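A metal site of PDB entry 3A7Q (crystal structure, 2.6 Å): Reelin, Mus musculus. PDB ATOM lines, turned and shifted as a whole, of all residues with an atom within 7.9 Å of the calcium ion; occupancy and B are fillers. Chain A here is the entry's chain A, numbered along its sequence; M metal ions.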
ATOM      1  N   ASP A  15      -6.596 -23.597 -24.005  1.00  0.00           N
ATOM      2  CA  ASP A  15      -7.736 -23.091 -23.221  1.00  0.00           C
ATOM      3  C   ASP A  15      -9.018 -22.951 -24.023  1.00  0.00           C
ATOM      4  O   ASP A  15      -9.107 -22.139 -24.934  1.00  0.00           O
ATOM      5  CB  ASP A  15      -7.395 -21.775 -22.482  1.00  0.00           C
ATOM      6  CG  ASP A  15      -8.146 -21.635 -21.150  1.00  0.00           C
ATOM      7  OD1 ASP A  15      -7.579 -21.041 -20.207  1.00  0.00           O
ATOM      8  OD2 ASP A  15      -9.295 -22.111 -21.046  1.00  0.00           O
ATOM      9  N   THR A  16     -10.006 -23.773 -23.688  1.00  0.00           N
ATOM     10  CA  THR A  16     -11.325 -23.743 -24.313  1.00  0.00           C
ATOM     11  C   THR A  16     -12.288 -22.838 -23.540  1.00  0.00           C
ATOM     12  O   THR A  16     -13.444 -22.677 -23.940  1.00  0.00           O
ATOM     13  CB  THR A  16     -11.934 -25.160 -24.465  1.00  0.00           C
ATOM     14  OG1 THR A  16     -11.961 -25.820 -23.202  1.00  0.00           O
ATOM     15  CG2 THR A  16     -11.106 -25.998 -25.426  1.00  0.00           C
ATOM     16  N   PHE A  17     -11.799 -22.235 -22.455  1.00  0.00           N
ATOM     17  CA  PHE A  17     -12.573 -21.399 -21.517  1.00  0.00           C
ATOM     18  C   PHE A  17     -13.929 -21.979 -21.147  1.00  0.00           C
ATOM     19  O   PHE A  17     -14.841 -21.240 -20.779  1.00  0.00           O
ATOM     20  CB  PHE A  17     -12.767 -19.991 -22.073  1.00  0.00           C
ATOM     21  CG  PHE A  17     -11.498 -19.303 -22.404  1.00  0.00           C
ATOM     22  CD1 PHE A  17     -11.032 -19.261 -23.718  1.00  0.00           C
ATOM     23  CD2 PHE A  17     -10.752 -18.662 -21.414  1.00  0.00           C
ATOM     24  CE1 PHE A  17      -9.853 -18.620 -24.033  1.00  0.00           C
ATOM     25  CE2 PHE A  17      -9.562 -18.015 -21.735  1.00  0.00           C
ATOM     26  CZ  PHE A  17      -9.112 -17.992 -23.049  1.00  0.00           C
ATOM     27  N   ASP A  18     -14.073 -23.290 -21.232  1.00  0.00           N
ATOM     28  CA  ASP A  18     -15.404 -23.829 -21.305  1.00  0.00           C
ATOM     29  C   ASP A  18     -16.149 -24.075 -19.983  1.00  0.00           C
ATOM     30  O   ASP A  18     -17.288 -24.520 -19.996  1.00  0.00           O
ATOM     31  CB  ASP A  18     -15.513 -24.981 -22.312  1.00  0.00           C
ATOM     32  CG  ASP A  18     -16.428 -24.635 -23.490  1.00  0.00           C
ATOM     33  OD1 ASP A  18     -17.567 -25.170 -23.509  1.00  0.00           O
ATOM     34  OD2 ASP A  18     -16.034 -23.805 -24.358  1.00  0.00           O
ATOM     35  N   PHE A  19     -15.491 -23.778 -18.849  1.00  0.00           N
ATOM     36  CA  PHE A  19     -16.188 -23.409 -17.607  1.00  0.00           C
ATOM     37  C   PHE A  19     -15.297 -22.559 -16.696  1.00  0.00           C
ATOM     38  O   PHE A  19     -15.099 -22.873 -15.524  1.00  0.00           O
ATOM     39  CB  PHE A  19     -16.898 -24.580 -16.865  1.00  0.00           C
ATOM     40  CG  PHE A  19     -15.983 -25.662 -16.326  1.00  0.00           C
ATOM     41  CD1 PHE A  19     -15.820 -26.872 -17.012  1.00  0.00           C
ATOM     42  CD2 PHE A  19     -15.331 -25.516 -15.092  1.00  0.00           C
ATOM     43  CE1 PHE A  19     -14.996 -27.883 -16.506  1.00  0.00           C
ATOM     44  CE2 PHE A  19     -14.502 -26.516 -14.580  1.00  0.00           C
ATOM     45  CZ  PHE A  19     -14.337 -27.705 -15.289  1.00  0.00           C
ATOM     46  N   GLY A  35     -18.153 -15.897 -20.950  1.00  0.00           N
ATOM     47  CA  GLY A  35     -19.538 -15.917 -21.410  1.00  0.00           C
ATOM     48  C   GLY A  35     -19.685 -16.143 -22.903  1.00  0.00           C
ATOM     49  O   GLY A  35     -18.819 -16.705 -23.560  1.00  0.00           O
ATOM     50  N   ASP A  49     -18.989 -22.594 -26.931  1.00  0.00           N
ATOM     51  CA  ASP A  49     -20.012 -21.768 -26.283  1.00  0.00           C
ATOM     52  C   ASP A  49     -19.405 -20.731 -25.330  1.00  0.00           C
ATOM     53  O   ASP A  49     -19.668 -19.529 -25.467  1.00  0.00           O
ATOM     54  CB  ASP A  49     -21.054 -22.636 -25.571  1.00  0.00           C
ATOM     55  CG  ASP A  49     -21.770 -23.600 -26.516  1.00  0.00           C
ATOM     56  OD1 ASP A  49     -22.753 -24.258 -26.077  1.00  0.00           O
ATOM     57  OD2 ASP A  49     -21.365 -23.712 -27.698  1.00  0.00           O
ATOM     58  N   SER A  50     -18.595 -21.161 -24.366  1.00  0.00           N
ATOM     59  CA  SER A  50     -17.935 -20.220 -23.464  1.00  0.00           C
ATOM     60  C   SER A  50     -16.710 -19.626 -24.134  1.00  0.00           C
ATOM     61  O   SER A  50     -15.888 -20.343 -24.733  1.00  0.00           O
ATOM     62  CB  SER A  50     -17.542 -20.883 -22.146  1.00  0.00           C
ATOM     63  OG  SER A  50     -18.586 -20.864 -21.184  1.00  0.00           O
ATOM     64  N   ALA A  51     -16.570 -18.306 -24.046  1.00  0.00           N
ATOM     65  CA  ALA A  51     -15.353 -17.641 -24.487  1.00  0.00           C
ATOM     66  C   ALA A  51     -14.938 -16.583 -23.488  1.00  0.00           C
ATOM     67  O   ALA A  51     -15.675 -16.256 -22.528  1.00  0.00           O
ATOM     68  CB  ALA A  51     -15.531 -17.038 -25.874  1.00  0.00           C
ATOM     69  N   MET A  52     -13.742 -16.059 -23.706  1.00  0.00           N
ATOM     70  CA  MET A  52     -13.203 -14.962 -22.929  1.00  0.00           C
ATOM     71  C   MET A  52     -13.562 -13.664 -23.634  1.00  0.00           C
ATOM     72  O   MET A  52     -12.927 -13.270 -24.616  1.00  0.00           O
ATOM     73  CB  MET A  52     -11.678 -15.104 -22.787  1.00  0.00           C
ATOM     74  CG  MET A  52     -11.036 -13.911 -22.047  1.00  0.00           C
ATOM     75  SD  MET A  52     -11.552 -13.894 -20.319  1.00  0.00           S
ATOM     76  CE  MET A  52     -10.378 -15.040 -19.597  1.00  0.00           C
ATOM     77  N   GLU A  80      -9.453 -18.822 -31.824  1.00  0.00           N
ATOM     78  CA  GLU A  80     -10.636 -18.233 -32.444  1.00  0.00           C
ATOM     79  C   GLU A  80     -10.834 -16.823 -31.890  1.00  0.00           C
ATOM     80  O   GLU A  80     -10.451 -16.541 -30.755  1.00  0.00           O
ATOM     81  CB  GLU A  80     -11.852 -19.091 -32.186  1.00  0.00           C
ATOM     82  CG  GLU A  80     -11.656 -20.518 -32.659  1.00  0.00           C
ATOM     83  CD  GLU A  80     -12.858 -21.398 -32.418  1.00  0.00           C
ATOM     84  OE1 GLU A  80     -13.712 -21.067 -31.570  1.00  0.00           O
ATOM     85  OE2 GLU A  80     -12.946 -22.458 -33.082  1.00  0.00           O
ATOM     86  N   TRP A 143     -17.250 -15.260 -35.894  1.00  0.00           N
ATOM     87  CA  TRP A 143     -15.988 -15.780 -35.405  1.00  0.00           C
ATOM     88  C   TRP A 143     -15.139 -16.346 -36.532  1.00  0.00           C
ATOM     89  O   TRP A 143     -15.647 -16.876 -37.513  1.00  0.00           O
ATOM     90  CB  TRP A 143     -16.276 -16.917 -34.436  1.00  0.00           C
ATOM     91  CG  TRP A 143     -16.812 -16.504 -33.097  1.00  0.00           C
ATOM     92  CD1 TRP A 143     -18.103 -16.193 -32.784  1.00  0.00           C
ATOM     93  CD2 TRP A 143     -16.054 -16.382 -31.884  1.00  0.00           C
ATOM     94  NE1 TRP A 143     -18.198 -15.880 -31.449  1.00  0.00           N
ATOM     95  CE2 TRP A 143     -16.967 -15.994 -30.869  1.00  0.00           C
ATOM     96  CE3 TRP A 143     -14.709 -16.554 -31.559  1.00  0.00           C
ATOM     97  CZ2 TRP A 143     -16.554 -15.773 -29.543  1.00  0.00           C
ATOM     98  CZ3 TRP A 143     -14.297 -16.337 -30.257  1.00  0.00           C
ATOM     99  CH2 TRP A 143     -15.226 -15.952 -29.258  1.00  0.00           C
ATOM    100  N   ILE A 179     -11.736 -13.789 -27.426  1.00  0.00           N
ATOM    101  CA  ILE A 179     -11.055 -14.997 -27.934  1.00  0.00           C
ATOM    102  C   ILE A 179     -11.621 -16.331 -27.397  1.00  0.00           C
ATOM    103  O   ILE A 179     -12.245 -16.385 -26.345  1.00  0.00           O
ATOM    104  CB  ILE A 179      -9.504 -15.003 -27.782  1.00  0.00           C
ATOM    105  CG1 ILE A 179      -9.082 -14.786 -26.323  1.00  0.00           C
ATOM    106  CG2 ILE A 179      -8.853 -13.986 -28.703  1.00  0.00           C
ATOM    107  CD1 ILE A 179      -7.529 -14.821 -26.117  1.00  0.00           C
ATOM    108  N   ASP A 180     -11.396 -17.400 -28.142  1.00  0.00           N
ATOM    109  CA  ASP A 180     -11.748 -18.728 -27.702  1.00  0.00           C
ATOM    110  C   ASP A 180     -10.716 -19.723 -28.210  1.00  0.00           C
ATOM    111  O   ASP A 180      -9.948 -19.408 -29.109  1.00  0.00           O
ATOM    112  CB  ASP A 180     -13.159 -19.070 -28.207  1.00  0.00           C
ATOM    113  CG  ASP A 180     -13.822 -20.143 -27.412  1.00  0.00           C
ATOM    114  OD1 ASP A 180     -13.167 -20.709 -26.540  1.00  0.00           O
ATOM    115  OD2 ASP A 180     -15.000 -20.440 -27.648  1.00  0.00           O
ATOM    116  N   ASN A 181     -10.697 -20.922 -27.624  1.00  0.00           N
ATOM    117  CA  ASN A 181      -9.932 -22.077 -28.135  1.00  0.00           C
ATOM    118  C   ASN A 181      -8.492 -21.768 -28.505  1.00  0.00           C
ATOM    119  O   ASN A 181      -8.092 -21.855 -29.666  1.00  0.00           O
ATOM    120  CB  ASN A 181     -10.650 -22.721 -29.321  1.00  0.00           C
ATOM    121  CG  ASN A 181     -12.061 -23.181 -28.977  1.00  0.00           C
ATOM    122  OD1 ASN A 181     -12.412 -23.342 -27.801  1.00  0.00           O
ATOM    123  ND2 ASN A 181     -12.869 -23.425 -29.998  1.00  0.00           N
ATOM    124  N   VAL A 182      -7.700 -21.437 -27.494  1.00  0.00           N
ATOM    125  CA  VAL A 182      -6.327 -20.985 -27.727  1.00  0.00           C
ATOM    126  C   VAL A 182      -5.324 -22.127 -27.583  1.00  0.00           C
ATOM    127  O   VAL A 182      -5.245 -22.770 -26.534  1.00  0.00           O
ATOM    128  CB  VAL A 182      -5.962 -19.815 -26.790  1.00  0.00           C
ATOM    129  CG1 VAL A 182      -4.519 -19.379 -27.015  1.00  0.00           C
ATOM    130  CG2 VAL A 182      -6.915 -18.654 -27.026  1.00  0.00           C
HETATM  131 CA    CA M   1     -14.990 -22.199 -25.729  1.00  0.00          CA
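The backbone carbonyl oxygen (O) of Ser 50 binds the calcium ion (2.3 Å). The calcium ion is bound by OD2 of Asp 18 (2.4 Å). The calcium ion is bound by O of Thr 16 (2.4 Å). The side-chain carboxylate (OD1) of Asp 180 is bound to the calcium ion (2.5 Å). The calcium ion is bound by OD2 of Asp 180 (2.6 Å).
The side-chain amide oxygen (OD1) of Asn 181 sits close to the side-chain carboxylate (OD1) of Asp 180 (3.0 Å). The backbone NH of Glu 80 lies within hydrogen-bond range of the backbone carbonyl oxygen of Asp 180, at 2.8 Å. O of Asp 15 lies close to N of Asn 181 (3.4 Å). The side-chain amide nitrogen (ND2) of Asn 181 lies within hydrogen-bond range of the side-chain carboxylate (OE1) of Glu 80.
Residues that only touch the calcium ion: Asn 181. Five residues have an atom within 4 Å of the calcium ion: Thr 16, Asp 18, Ser 50, Asp 180 and Asn 181.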
